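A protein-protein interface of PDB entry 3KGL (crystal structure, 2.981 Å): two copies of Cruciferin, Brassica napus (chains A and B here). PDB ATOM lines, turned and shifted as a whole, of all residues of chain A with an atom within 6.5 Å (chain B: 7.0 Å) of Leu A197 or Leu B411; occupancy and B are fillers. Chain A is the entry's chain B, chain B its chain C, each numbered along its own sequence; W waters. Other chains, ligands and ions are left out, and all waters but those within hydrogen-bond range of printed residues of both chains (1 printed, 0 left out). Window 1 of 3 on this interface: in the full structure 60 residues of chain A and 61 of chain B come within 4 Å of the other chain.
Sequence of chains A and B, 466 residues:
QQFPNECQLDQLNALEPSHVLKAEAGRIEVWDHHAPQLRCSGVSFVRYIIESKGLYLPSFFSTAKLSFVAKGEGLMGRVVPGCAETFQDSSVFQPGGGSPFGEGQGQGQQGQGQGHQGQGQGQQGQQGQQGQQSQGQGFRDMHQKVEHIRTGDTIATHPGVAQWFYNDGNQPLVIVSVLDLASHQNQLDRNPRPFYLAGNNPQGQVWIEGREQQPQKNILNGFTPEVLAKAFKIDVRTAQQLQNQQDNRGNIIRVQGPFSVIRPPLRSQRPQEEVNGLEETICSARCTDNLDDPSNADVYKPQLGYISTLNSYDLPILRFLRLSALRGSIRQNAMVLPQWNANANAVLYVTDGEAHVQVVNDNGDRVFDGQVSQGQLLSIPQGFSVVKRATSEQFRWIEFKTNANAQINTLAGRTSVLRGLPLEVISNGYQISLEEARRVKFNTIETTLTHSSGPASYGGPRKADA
Water W1 lies within hydrogen-bond range of ND2 of Asn A244 (2.7 Å) and O of Tyr B430 (2.9 Å).
ND2 of Asn A244 is in hydrogen-bond range of O of Tyr B430.
O of Leu A197 is in hydrogen-bond range of OH of Tyr B430 (2.7 Å).
No position is printed for both chains.
Of the 16 pairs that touch across the chains among the printed residues, none has its exchanged pair printed and touching as well.
Among the printed residues, merely in contact across the chains: Phe A232 with Leu B411 (2.9 Å), Leu A242 with Tyr B430 (3.1 Å), Leu A220 with Tyr B430 (3.3 Å), Phe A232 with Ala B412 (3.3 Å), Phe A60 with Trp B340 (3.4 Å), Leu A197 with Val B417 (3.5 Å), Ile A219 with Ser B385 (3.6 Å), Phe A223 with Ser B385 (3.6 Å), Phe A232 with Val B440 (3.6 Å), Ala A162 with Val B417 (3.7 Å), Phe A232 with Leu B418 (3.7 Å), Ala A198 with Tyr B430 (3.8 Å), Leu A242 with Val B440 (3.96 Å) and Leu A197 with Leu B411 (3.99 Å).
Of the 18 printed residues of chain A, 10 touch a printed residue of chain B.
Printed residues of chain A that touch a printed residue of chain B: Phe A60, Ala A162, Leu A197, Ala A198, Ile A219, Leu A220, Phe A223, Phe A232, Leu A242 and Asn A244.
Hydrophobic or aromatic side chains of chain A that line the printed part of chain B: Phe A60, Ala A162, Leu A197, Ala A198, Ile A219, Leu A220, Phe A223, Phe A232 and Leu A242.
Printed residues of chain B that touch a printed residue of chain A: Trp B340, Ser B385, Leu B411, Ala B412, Val B417, Leu B418, Tyr B430 and Val B440.
Among the printed residues, no Asp or Glu carboxylate lies within 4 Å of a Lys or Arg side-chain nitrogen of the other chain.
Of the printed residues of chain B, Leu A197 touches Leu B411 (3.99 Å), Val B417 (3.5 Å) and Tyr B430 (2.7 Å).
Of the printed residues of chain A, Leu B418 touches Phe A232.
Of the printed residues of chain A, Tyr B430 touches Leu A197 (2.7 Å), Ala A198 (3.8 Å), Leu A220 (3.3 Å), Leu A242 (3.1 Å) and Asn A244 (3.4 Å).
Of the printed residues of chain A, Ser B385 touches Ile A219 (3.6 Å) and Phe A223 (3.6 Å).
Printed residues of chain A within 4 Å of Val B440: Phe A232 and Leu A242.
The nearest printed residue of chain B that does not touch Leu A197 is Trp B340 (4.5 Å).
The backbone carbonyl oxygen (O) of Pro A58 sits at hydrogen-bond distance from the backbone NH (N) of Leu A197 (3.0 Å).
The backbone NH (N) of Leu B411 lies within hydrogen-bond range of the backbone carbonyl oxygen (O) of Pro B338.
The backbone NH of Phe A195 lies within hydrogen-bond range of the backbone carbonyl oxygen of Phe A60 (2.8 Å).
The backbone NH (N) of Ile A219 lies within hydrogen-bond range of the backbone carbonyl oxygen (O) of Tyr A196 (2.8 Å).
The backbone carbonyl oxygen (O) of Thr B410 is in hydrogen-bond range of the backbone NH (N) of Val B417.
ND2 of Asn A218 lies within hydrogen-bond range of O of Ala A198, 2.6 Å away.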
ATOM      1  N   LEU A  57      -5.994 -30.259 -28.424  1.00  0.00           N
ATOM      2  CA  LEU A  57      -6.227 -30.661 -27.038  1.00  0.00           C
ATOM      3  C   LEU A  57      -7.284 -29.808 -26.376  1.00  0.00           C
ATOM      4  O   LEU A  57      -7.415 -28.621 -26.676  1.00  0.00           O
ATOM      5  CB  LEU A  57      -4.938 -30.630 -26.230  1.00  0.00           C
ATOM      6  CG  LEU A  57      -3.837 -31.558 -26.743  1.00  0.00           C
ATOM      7  CD1 LEU A  57      -2.576 -31.372 -25.938  1.00  0.00           C
ATOM      8  CD2 LEU A  57      -4.286 -33.000 -26.694  1.00  0.00           C
ATOM      9  N   PRO A  58      -8.036 -30.414 -25.453  1.00  0.00           N
ATOM     10  CA  PRO A  58      -9.181 -29.779 -24.793  1.00  0.00           C
ATOM     11  C   PRO A  58      -8.888 -28.369 -24.255  1.00  0.00           C
ATOM     12  O   PRO A  58      -7.874 -28.094 -23.602  1.00  0.00           O
ATOM     13  CB  PRO A  58      -9.501 -30.744 -23.638  1.00  0.00           C
ATOM     14  CG  PRO A  58      -8.981 -32.032 -24.073  1.00  0.00           C
ATOM     15  CD  PRO A  58      -7.731 -31.720 -24.860  1.00  0.00           C
ATOM     16  N   SER A  59      -9.814 -27.471 -24.548  1.00  0.00           N
ATOM     17  CA  SER A  59      -9.741 -26.120 -24.051  1.00  0.00           C
ATOM     18  C   SER A  59     -11.160 -25.668 -23.825  1.00  0.00           C
ATOM     19  O   SER A  59     -12.109 -26.369 -24.166  1.00  0.00           O
ATOM     20  CB  SER A  59      -9.038 -25.195 -25.052  1.00  0.00           C
ATOM     21  OG  SER A  59      -9.815 -24.999 -26.228  1.00  0.00           O
ATOM     22  N   PHE A  60     -11.297 -24.498 -23.220  1.00  0.00           N
ATOM     23  CA  PHE A  60     -12.593 -23.903 -23.011  1.00  0.00           C
ATOM     24  C   PHE A  60     -12.409 -22.403 -22.932  1.00  0.00           C
ATOM     25  O   PHE A  60     -11.304 -21.907 -22.700  1.00  0.00           O
ATOM     26  CB  PHE A  60     -13.282 -24.482 -21.767  1.00  0.00           C
ATOM     27  CG  PHE A  60     -12.681 -24.047 -20.451  1.00  0.00           C
ATOM     28  CD1 PHE A  60     -13.062 -22.853 -19.858  1.00  0.00           C
ATOM     29  CD2 PHE A  60     -11.777 -24.851 -19.782  1.00  0.00           C
ATOM     30  CE1 PHE A  60     -12.529 -22.462 -18.635  1.00  0.00           C
ATOM     31  CE2 PHE A  60     -11.242 -24.463 -18.559  1.00  0.00           C
ATOM     32  CZ  PHE A  60     -11.622 -23.272 -17.988  1.00  0.00           C
ATOM     33  N   ALA A 162     -15.541 -27.298 -22.492  1.00  0.00           N
ATOM     34  CA  ALA A 162     -14.341 -27.864 -23.087  1.00  0.00           C
ATOM     35  C   ALA A 162     -14.661 -28.535 -24.423  1.00  0.00           C
ATOM     36  O   ALA A 162     -15.742 -29.091 -24.605  1.00  0.00           O
ATOM     37  CB  ALA A 162     -13.716 -28.866 -22.136  1.00  0.00           C
ATOM     38  N   PHE A 195      -8.581 -21.338 -22.258  1.00  0.00           N
ATOM     39  CA  PHE A 195      -8.020 -22.020 -21.094  1.00  0.00           C
ATOM     40  C   PHE A 195      -7.640 -23.432 -21.515  1.00  0.00           C
ATOM     41  O   PHE A 195      -8.513 -24.249 -21.794  1.00  0.00           O
ATOM     42  CB  PHE A 195      -9.057 -22.108 -19.971  1.00  0.00           C
ATOM     43  CG  PHE A 195      -9.342 -20.797 -19.293  1.00  0.00           C
ATOM     44  CD1 PHE A 195      -8.736 -20.476 -18.099  1.00  0.00           C
ATOM     45  CD2 PHE A 195     -10.225 -19.897 -19.842  1.00  0.00           C
ATOM     46  CE1 PHE A 195      -8.997 -19.277 -17.478  1.00  0.00           C
ATOM     47  CE2 PHE A 195     -10.487 -18.704 -19.226  1.00  0.00           C
ATOM     48  CZ  PHE A 195      -9.877 -18.394 -18.042  1.00  0.00           C
ATOM     49  N   TYR A 196      -6.347 -23.732 -21.572  1.00  0.00           N
ATOM     50  CA  TYR A 196      -5.929 -25.054 -22.026  1.00  0.00           C
ATOM     51  C   TYR A 196      -5.867 -26.068 -20.900  1.00  0.00           C
ATOM     52  O   TYR A 196      -5.215 -25.832 -19.881  1.00  0.00           O
ATOM     53  CB  TYR A 196      -4.591 -24.986 -22.756  1.00  0.00           C
ATOM     54  CG  TYR A 196      -4.653 -24.154 -24.017  1.00  0.00           C
ATOM     55  CD1 TYR A 196      -5.544 -24.468 -25.037  1.00  0.00           C
ATOM     56  CD2 TYR A 196      -3.838 -23.053 -24.182  1.00  0.00           C
ATOM     57  CE1 TYR A 196      -5.607 -23.714 -26.188  1.00  0.00           C
ATOM     58  CE2 TYR A 196      -3.901 -22.292 -25.325  1.00  0.00           C
ATOM     59  CZ  TYR A 196      -4.778 -22.628 -26.325  1.00  0.00           C
ATOM     60  OH  TYR A 196      -4.818 -21.873 -27.470  1.00  0.00           O
ATOM     61  N   LEU A 197      -6.550 -27.198 -21.093  1.00  0.00           N
ATOM     62  CA  LEU A 197      -6.491 -28.313 -20.149  1.00  0.00           C
ATOM     63  C   LEU A 197      -5.231 -29.191 -20.295  1.00  0.00           C
ATOM     64  O   LEU A 197      -4.784 -29.789 -19.329  1.00  0.00           O
ATOM     65  CB  LEU A 197      -7.745 -29.162 -20.259  1.00  0.00           C
ATOM     66  CG  LEU A 197      -8.880 -28.927 -19.265  1.00  0.00           C
ATOM     67  CD1 LEU A 197      -8.907 -27.507 -18.785  1.00  0.00           C
ATOM     68  CD2 LEU A 197     -10.187 -29.280 -19.917  1.00  0.00           C
ATOM     69  N   ALA A 198      -4.635 -29.259 -21.484  1.00  0.00           N
ATOM     70  CA  ALA A 198      -3.443 -30.087 -21.641  1.00  0.00           C
ATOM     71  C   ALA A 198      -2.249 -29.404 -22.292  1.00  0.00           C
ATOM     72  O   ALA A 198      -1.136 -29.457 -21.764  1.00  0.00           O
ATOM     73  CB  ALA A 198      -3.786 -31.368 -22.391  1.00  0.00           C
ATOM     74  N   GLY A 199      -2.470 -28.787 -23.448  1.00  0.00           N
ATOM     75  CA  GLY A 199      -1.377 -28.211 -24.210  1.00  0.00           C
ATOM     76  C   GLY A 199      -0.562 -27.119 -23.526  1.00  0.00           C
ATOM     77  O   GLY A 199      -1.065 -26.331 -22.713  1.00  0.00           O
ATOM     78  N   ASN A 218      -0.578 -25.017 -19.443  1.00  0.00           N
ATOM     79  CA  ASN A 218      -1.935 -25.451 -19.198  1.00  0.00           C
ATOM     80  C   ASN A 218      -2.396 -25.142 -17.783  1.00  0.00           C
ATOM     81  O   ASN A 218      -1.590 -24.899 -16.883  1.00  0.00           O
ATOM     82  CB  ASN A 218      -2.099 -26.936 -19.516  1.00  0.00           C
ATOM     83  CG  ASN A 218      -1.248 -27.833 -18.637  1.00  0.00           C
ATOM     84  OD1 ASN A 218      -0.916 -27.501 -17.495  1.00  0.00           O
ATOM     85  ND2 ASN A 218      -0.909 -29.000 -19.168  1.00  0.00           N
ATOM     86  N   ILE A 219      -3.708 -25.153 -17.614  1.00  0.00           N
ATOM     87  CA  ILE A 219      -4.346 -24.919 -16.328  1.00  0.00           C
ATOM     88  C   ILE A 219      -3.714 -25.715 -15.203  1.00  0.00           C
ATOM     89  O   ILE A 219      -3.535 -25.209 -14.105  1.00  0.00           O
ATOM     90  CB  ILE A 219      -5.833 -25.282 -16.393  1.00  0.00           C
ATOM     91  CG1 ILE A 219      -6.526 -24.420 -17.442  1.00  0.00           C
ATOM     92  CG2 ILE A 219      -6.479 -25.087 -15.062  1.00  0.00           C
ATOM     93  CD1 ILE A 219      -6.003 -22.995 -17.482  1.00  0.00           C
ATOM     94  N   LEU A 220      -3.374 -26.967 -15.475  1.00  0.00           N
ATOM     95  CA  LEU A 220      -2.846 -27.838 -14.432  1.00  0.00           C
ATOM     96  C   LEU A 220      -1.465 -27.371 -13.935  1.00  0.00           C
ATOM     97  O   LEU A 220      -1.102 -27.611 -12.781  1.00  0.00           O
ATOM     98  CB  LEU A 220      -2.815 -29.283 -14.926  1.00  0.00           C
ATOM     99  CG  LEU A 220      -4.094 -30.127 -14.813  1.00  0.00           C
ATOM    100  CD1 LEU A 220      -5.365 -29.337 -14.742  1.00  0.00           C
ATOM    101  CD2 LEU A 220      -4.185 -31.081 -15.961  1.00  0.00           C
ATOM    102  N   PHE A 223      -1.154 -25.130 -10.686  1.00  0.00           N
ATOM    103  CA  PHE A 223      -1.230 -25.702  -9.366  1.00  0.00           C
ATOM    104  C   PHE A 223       0.112 -26.300  -9.002  1.00  0.00           C
ATOM    105  O   PHE A 223       0.907 -26.627  -9.883  1.00  0.00           O
ATOM    106  CB  PHE A 223      -2.298 -26.775  -9.331  1.00  0.00           C
ATOM    107  CG  PHE A 223      -3.678 -26.253  -9.541  1.00  0.00           C
ATOM    108  CD1 PHE A 223      -4.436 -25.820  -8.473  1.00  0.00           C
ATOM    109  CD2 PHE A 223      -4.219 -26.194 -10.804  1.00  0.00           C
ATOM    110  CE1 PHE A 223      -5.708 -25.344  -8.665  1.00  0.00           C
ATOM    111  CE2 PHE A 223      -5.499 -25.720 -11.000  1.00  0.00           C
ATOM    112  CZ  PHE A 223      -6.241 -25.295  -9.933  1.00  0.00           C
ATOM    113  N   PHE A 232      -6.227 -35.843  -7.530  1.00  0.00           N
ATOM    114  CA  PHE A 232      -6.455 -36.823  -8.580  1.00  0.00           C
ATOM    115  C   PHE A 232      -6.191 -38.198  -8.018  1.00  0.00           C
ATOM    116  O   PHE A 232      -6.557 -39.215  -8.620  1.00  0.00           O
ATOM    117  CB  PHE A 232      -5.468 -36.599  -9.727  1.00  0.00           C
ATOM    118  CG  PHE A 232      -5.847 -35.484 -10.648  1.00  0.00           C
ATOM    119  CD1 PHE A 232      -6.926 -35.616 -11.509  1.00  0.00           C
ATOM    120  CD2 PHE A 232      -5.111 -34.305 -10.672  1.00  0.00           C
ATOM    121  CE1 PHE A 232      -7.276 -34.597 -12.364  1.00  0.00           C
ATOM    122  CE2 PHE A 232      -5.452 -33.270 -11.533  1.00  0.00           C
ATOM    123  CZ  PHE A 232      -6.539 -33.419 -12.378  1.00  0.00           C
ATOM    124  N   LEU A 242       1.434 -34.115 -16.042  1.00  0.00           N
ATOM    125  CA  LEU A 242       0.248 -33.453 -16.563  1.00  0.00           C
ATOM    126  C   LEU A 242       0.483 -31.973 -16.720  1.00  0.00           C
ATOM    127  O   LEU A 242      -0.321 -31.291 -17.344  1.00  0.00           O
ATOM    128  CB  LEU A 242      -0.939 -33.651 -15.620  1.00  0.00           C
ATOM    129  CG  LEU A 242      -1.200 -35.043 -15.062  1.00  0.00           C
ATOM    130  CD1 LEU A 242      -2.040 -34.916 -13.804  1.00  0.00           C
ATOM    131  CD2 LEU A 242      -1.874 -35.932 -16.105  1.00  0.00           C
ATOM    132  N   ASN A 244       2.782 -30.585 -18.307  1.00  0.00           N
ATOM    133  CA  ASN A 244       3.421 -30.348 -19.598  1.00  0.00           C
ATOM    134  C   ASN A 244       4.429 -29.197 -19.620  1.00  0.00           C
ATOM    135  O   ASN A 244       4.538 -28.466 -20.609  1.00  0.00           O
ATOM    136  CB  ASN A 244       2.391 -30.220 -20.721  1.00  0.00           C
ATOM    137  CG  ASN A 244       1.907 -31.577 -21.227  1.00  0.00           C
ATOM    138  OD1 ASN A 244       0.751 -31.716 -21.636  1.00  0.00           O
ATOM    139  ND2 ASN A 244       2.793 -32.584 -21.203  1.00  0.00           N
ATOM    140  N   ASN A 251      -0.730 -26.894 -28.904  1.00  0.00           N
ATOM    141  CA  ASN A 251      -2.016 -27.466 -28.522  1.00  0.00           C
ATOM    142  C   ASN A 251      -2.572 -28.469 -29.511  1.00  0.00           C
ATOM    143  O   ASN A 251      -3.479 -29.233 -29.184  1.00  0.00           O
ATOM    144  CB  ASN A 251      -3.064 -26.397 -28.259  1.00  0.00           C
ATOM    145  CG  ASN A 251      -4.161 -26.896 -27.360  1.00  0.00           C
ATOM    146  OD1 ASN A 251      -5.314 -26.993 -27.766  1.00  0.00           O
ATOM    147  ND2 ASN A 251      -3.801 -27.248 -26.132  1.00  0.00           N
ATOM    148  N   LEU B 337     -12.104 -30.051  -4.331  1.00  0.00           N
ATOM    149  CA  LEU B 337     -11.427 -30.391  -5.575  1.00  0.00           C
ATOM    150  C   LEU B 337     -11.379 -29.212  -6.547  1.00  0.00           C
ATOM    151  O   LEU B 337     -12.355 -28.471  -6.691  1.00  0.00           O
ATOM    152  CB  LEU B 337     -12.135 -31.569  -6.240  1.00  0.00           C
ATOM    153  CG  LEU B 337     -11.974 -32.972  -5.675  1.00  0.00           C
ATOM    154  CD1 LEU B 337     -12.972 -33.899  -6.364  1.00  0.00           C
ATOM    155  CD2 LEU B 337     -10.533 -33.488  -5.832  1.00  0.00           C
ATOM    156  N   PRO B 338     -10.241 -29.040  -7.222  1.00  0.00           N
ATOM    157  CA  PRO B 338     -10.063 -27.988  -8.230  1.00  0.00           C
ATOM    158  C   PRO B 338     -11.289 -27.799  -9.121  1.00  0.00           C
ATOM    159  O   PRO B 338     -11.699 -28.733  -9.803  1.00  0.00           O
ATOM    160  CB  PRO B 338      -8.876 -28.501  -9.047  1.00  0.00           C
ATOM    161  CG  PRO B 338      -8.044 -29.201  -8.027  1.00  0.00           C
ATOM    162  CD  PRO B 338      -9.021 -29.845  -7.049  1.00  0.00           C
ATOM    163  N   GLN B 339     -11.861 -26.598  -9.111  1.00  0.00           N
ATOM    164  CA  GLN B 339     -13.079 -26.301  -9.871  1.00  0.00           C
ATOM    165  C   GLN B 339     -12.969 -24.931 -10.528  1.00  0.00           C
ATOM    166  O   GLN B 339     -12.160 -24.109 -10.102  1.00  0.00           O
ATOM    167  CB  GLN B 339     -14.321 -26.345  -8.955  1.00  0.00           C
ATOM    168  CG  GLN B 339     -14.452 -25.174  -7.957  1.00  0.00           C
ATOM    169  CD  GLN B 339     -15.513 -25.401  -6.891  1.00  0.00           C
ATOM    170  OE1 GLN B 339     -16.022 -24.448  -6.283  1.00  0.00           O
ATOM    171  NE2 GLN B 339     -15.853 -26.670  -6.654  1.00  0.00           N
ATOM    172  N   TRP B 340     -13.773 -24.695 -11.563  1.00  0.00           N
ATOM    173  CA  TRP B 340     -13.920 -23.363 -12.153  1.00  0.00           C
ATOM    174  C   TRP B 340     -15.379 -23.097 -12.516  1.00  0.00           C
ATOM    175  O   TRP B 340     -16.119 -24.024 -12.823  1.00  0.00           O
ATOM    176  CB  TRP B 340     -13.024 -23.205 -13.383  1.00  0.00           C
ATOM    177  CG  TRP B 340     -13.629 -23.707 -14.654  1.00  0.00           C
ATOM    178  CD1 TRP B 340     -14.565 -23.082 -15.414  1.00  0.00           C
ATOM    179  CD2 TRP B 340     -13.320 -24.930 -15.330  1.00  0.00           C
ATOM    180  NE1 TRP B 340     -14.878 -23.846 -16.512  1.00  0.00           N
ATOM    181  CE2 TRP B 340     -14.122 -24.988 -16.484  1.00  0.00           C
ATOM    182  CE3 TRP B 340     -12.442 -25.989 -15.068  1.00  0.00           C
ATOM    183  CZ2 TRP B 340     -14.086 -26.048 -17.368  1.00  0.00           C
ATOM    184  CZ3 TRP B 340     -12.403 -27.045 -15.950  1.00  0.00           C
ATOM    185  CH2 TRP B 340     -13.222 -27.070 -17.084  1.00  0.00           C
ATOM    186  N   SER B 385      -9.299 -21.327 -12.001  1.00  0.00           N
ATOM    187  CA  SER B 385      -9.475 -22.555 -11.251  1.00  0.00           C
ATOM    188  C   SER B 385      -9.050 -22.412  -9.789  1.00  0.00           C
ATOM    189  O   SER B 385      -8.096 -21.699  -9.483  1.00  0.00           O
ATOM    190  CB  SER B 385      -8.733 -23.688 -11.941  1.00  0.00           C
ATOM    191  OG  SER B 385      -9.289 -23.893 -13.229  1.00  0.00           O
ATOM    192  N   VAL B 386      -9.773 -23.086  -8.893  1.00  0.00           N
ATOM    193  CA  VAL B 386      -9.605 -22.875  -7.464  1.00  0.00           C
ATOM    194  C   VAL B 386      -9.621 -24.164  -6.676  1.00  0.00           C
ATOM    195  O   VAL B 386     -10.622 -24.877  -6.650  1.00  0.00           O
ATOM    196  CB  VAL B 386     -10.758 -22.056  -6.872  1.00  0.00           C
ATOM    197  CG1 VAL B 386     -10.240 -21.124  -5.780  1.00  0.00           C
ATOM    198  CG2 VAL B 386     -11.501 -21.297  -7.961  1.00  0.00           C
ATOM    199  N   ASN B 409     -17.286 -26.521 -12.836  1.00  0.00           N
ATOM    200  CA  ASN B 409     -16.654 -27.567 -13.609  1.00  0.00           C
ATOM    201  C   ASN B 409     -15.462 -28.079 -12.840  1.00  0.00           C
ATOM    202  O   ASN B 409     -14.675 -27.322 -12.286  1.00  0.00           O
ATOM    203  CB  ASN B 409     -16.236 -27.073 -14.998  1.00  0.00           C
ATOM    204  CG  ASN B 409     -17.176 -27.543 -16.099  1.00  0.00           C
ATOM    205  OD1 ASN B 409     -17.215 -28.734 -16.438  1.00  0.00           O
ATOM    206  ND2 ASN B 409     -17.923 -26.605 -16.679  1.00  0.00           N
ATOM    207  N   THR B 410     -15.336 -29.386 -12.793  1.00  0.00           N
ATOM    208  CA  THR B 410     -14.376 -29.976 -11.907  1.00  0.00           C
ATOM    209  C   THR B 410     -13.222 -30.524 -12.739  1.00  0.00           C
ATOM    210  O   THR B 410     -13.433 -31.047 -13.822  1.00  0.00           O
ATOM    211  CB  THR B 410     -15.105 -30.989 -10.997  1.00  0.00           C
ATOM    212  OG1 THR B 410     -15.207 -30.421  -9.689  1.00  0.00           O
ATOM    213  CG2 THR B 410     -14.400 -32.320 -10.920  1.00  0.00           C
ATOM    214  N   LEU B 411     -12.000 -30.352 -12.262  1.00  0.00           N
ATOM    215  CA  LEU B 411     -10.836 -30.848 -12.982  1.00  0.00           C
ATOM    216  C   LEU B 411     -10.418 -32.226 -12.475  1.00  0.00           C
ATOM    217  O   LEU B 411      -9.472 -32.824 -12.983  1.00  0.00           O
ATOM    218  CB  LEU B 411      -9.661 -29.883 -12.842  1.00  0.00           C
ATOM    219  CG  LEU B 411      -9.763 -28.492 -13.469  1.00  0.00           C
ATOM    220  CD1 LEU B 411      -8.887 -27.536 -12.679  1.00  0.00           C
ATOM    221  CD2 LEU B 411      -9.387 -28.498 -14.955  1.00  0.00           C
ATOM    222  N   ALA B 412     -11.121 -32.726 -11.465  1.00  0.00           N
ATOM    223  CA  ALA B 412     -10.807 -34.033 -10.906  1.00  0.00           C
ATOM    224  C   ALA B 412     -11.981 -34.555 -10.095  1.00  0.00           C
ATOM    225  O   ALA B 412     -12.591 -33.811  -9.340  1.00  0.00           O
ATOM    226  CB  ALA B 412      -9.555 -33.950 -10.044  1.00  0.00           C
ATOM    227  N   GLY B 413     -12.295 -35.835 -10.249  1.00  0.00           N
ATOM    228  CA  GLY B 413     -13.394 -36.425  -9.514  1.00  0.00           C
ATOM    229  C   GLY B 413     -14.322 -37.137 -10.462  1.00  0.00           C
ATOM    230  O   GLY B 413     -14.007 -37.282 -11.635  1.00  0.00           O
ATOM    231  N   THR B 415     -17.176 -36.213 -11.544  1.00  0.00           N
ATOM    232  CA  THR B 415     -17.806 -35.261 -12.471  1.00  0.00           C
ATOM    233  C   THR B 415     -16.778 -34.522 -13.328  1.00  0.00           C
ATOM    234  O   THR B 415     -17.143 -33.674 -14.137  1.00  0.00           O
ATOM    235  CB  THR B 415     -18.591 -34.167 -11.728  1.00  0.00           C
ATOM    236  OG1 THR B 415     -17.716 -33.494 -10.807  1.00  0.00           O
ATOM    237  CG2 THR B 415     -19.780 -34.749 -10.986  1.00  0.00           C
ATOM    238  N   SER B 416     -15.499 -34.833 -13.140  1.00  0.00           N
ATOM    239  CA  SER B 416     -14.427 -34.062 -13.755  1.00  0.00           C
ATOM    240  C   SER B 416     -14.616 -33.885 -15.247  1.00  0.00           C
ATOM    241  O   SER B 416     -15.424 -34.578 -15.867  1.00  0.00           O
ATOM    242  CB  SER B 416     -13.057 -34.678 -13.460  1.00  0.00           C
ATOM    243  OG  SER B 416     -12.822 -35.829 -14.241  1.00  0.00           O
ATOM    244  N   VAL B 417     -13.885 -32.937 -15.821  1.00  0.00           N
ATOM    245  CA  VAL B 417     -13.943 -32.730 -17.256  1.00  0.00           C
ATOM    246  C   VAL B 417     -13.079 -33.821 -17.883  1.00  0.00           C
ATOM    247  O   VAL B 417     -13.231 -34.162 -19.058  1.00  0.00           O
ATOM    248  CB  VAL B 417     -13.447 -31.317 -17.663  1.00  0.00           C
ATOM    249  CG1 VAL B 417     -11.952 -31.236 -17.546  1.00  0.00           C
ATOM    250  CG2 VAL B 417     -13.859 -30.989 -19.080  1.00  0.00           C
ATOM    251  N   LEU B 418     -12.186 -34.388 -17.077  1.00  0.00           N
ATOM    252  CA  LEU B 418     -11.276 -35.411 -17.567  1.00  0.00           C
ATOM    253  C   LEU B 418     -11.964 -36.768 -17.637  1.00  0.00           C
ATOM    254  O   LEU B 418     -11.532 -37.671 -18.353  1.00  0.00           O
ATOM    255  CB  LEU B 418     -10.037 -35.476 -16.683  1.00  0.00           C
ATOM    256  CG  LEU B 418      -8.809 -34.723 -17.192  1.00  0.00           C
ATOM    257  CD1 LEU B 418      -9.172 -33.407 -17.860  1.00  0.00           C
ATOM    258  CD2 LEU B 418      -7.857 -34.485 -16.056  1.00  0.00           C
ATOM    259  N   ARG B 419     -13.045 -36.896 -16.882  1.00  0.00           N
ATOM    260  CA  ARG B 419     -13.858 -38.090 -16.889  1.00  0.00           C
ATOM    261  C   ARG B 419     -14.451 -38.235 -18.274  1.00  0.00           C
ATOM    262  O   ARG B 419     -14.441 -39.309 -18.856  1.00  0.00           O
ATOM    263  CB  ARG B 419     -14.986 -37.933 -15.879  1.00  0.00           C
ATOM    264  CG  ARG B 419     -15.475 -39.218 -15.267  1.00  0.00           C
ATOM    265  CD  ARG B 419     -14.765 -39.487 -13.966  1.00  0.00           C
ATOM    266  NE  ARG B 419     -15.255 -40.701 -13.330  1.00  0.00           N
ATOM    267  CZ  ARG B 419     -14.576 -41.372 -12.408  1.00  0.00           C
ATOM    268  NH1 ARG B 419     -13.378 -40.932 -12.027  1.00  0.00           N
ATOM    269  NH2 ARG B 419     -15.090 -42.480 -11.875  1.00  0.00           N
ATOM    270  N   LEU B 421     -13.389 -37.186 -20.992  1.00  0.00           N
ATOM    271  CA  LEU B 421     -12.377 -37.306 -22.035  1.00  0.00           C
ATOM    272  C   LEU B 421     -12.075 -38.778 -22.390  1.00  0.00           C
ATOM    273  O   LEU B 421     -11.810 -39.602 -21.515  1.00  0.00           O
ATOM    274  CB  LEU B 421     -11.083 -36.621 -21.586  1.00  0.00           C
ATOM    275  CG  LEU B 421     -10.660 -35.243 -22.100  1.00  0.00           C
ATOM    276  CD1 LEU B 421     -11.837 -34.342 -22.408  1.00  0.00           C
ATOM    277  CD2 LEU B 421      -9.740 -34.607 -21.080  1.00  0.00           C
ATOM    278  N   TYR B 430      -1.086 -35.550 -22.231  1.00  0.00           N
ATOM    279  CA  TYR B 430      -0.087 -35.273 -21.198  1.00  0.00           C
ATOM    280  C   TYR B 430       1.178 -36.092 -21.376  1.00  0.00           C
ATOM    281  O   TYR B 430       2.162 -35.925 -20.642  1.00  0.00           O
ATOM    282  CB  TYR B 430      -0.676 -35.507 -19.814  1.00  0.00           C
ATOM    283  CG  TYR B 430      -1.887 -34.652 -19.538  1.00  0.00           C
ATOM    284  CD1 TYR B 430      -1.758 -33.342 -19.098  1.00  0.00           C
ATOM    285  CD2 TYR B 430      -3.160 -35.154 -19.727  1.00  0.00           C
ATOM    286  CE1 TYR B 430      -2.871 -32.568 -18.854  1.00  0.00           C
ATOM    287  CE2 TYR B 430      -4.275 -34.389 -19.489  1.00  0.00           C
ATOM    288  CZ  TYR B 430      -4.132 -33.099 -19.055  1.00  0.00           C
ATOM    289  OH  TYR B 430      -5.268 -32.352 -18.818  1.00  0.00           O
ATOM    290  N   VAL B 440      -5.650 -41.149 -13.537  1.00  0.00           N
ATOM    291  CA  VAL B 440      -5.918 -39.713 -13.614  1.00  0.00           C
ATOM    292  C   VAL B 440      -7.389 -39.427 -13.959  1.00  0.00           C
ATOM    293  O   VAL B 440      -7.938 -38.370 -13.618  1.00  0.00           O
ATOM    294  CB  VAL B 440      -4.984 -39.041 -14.633  1.00  0.00           C
ATOM    295  CG1 VAL B 440      -5.555 -37.724 -15.092  1.00  0.00           C
ATOM    296  CG2 VAL B 440      -3.583 -38.849 -14.047  1.00  0.00           C
HETATM  297  O   HOH W   1       4.539 -34.365 -20.088  1.00  0.00           O
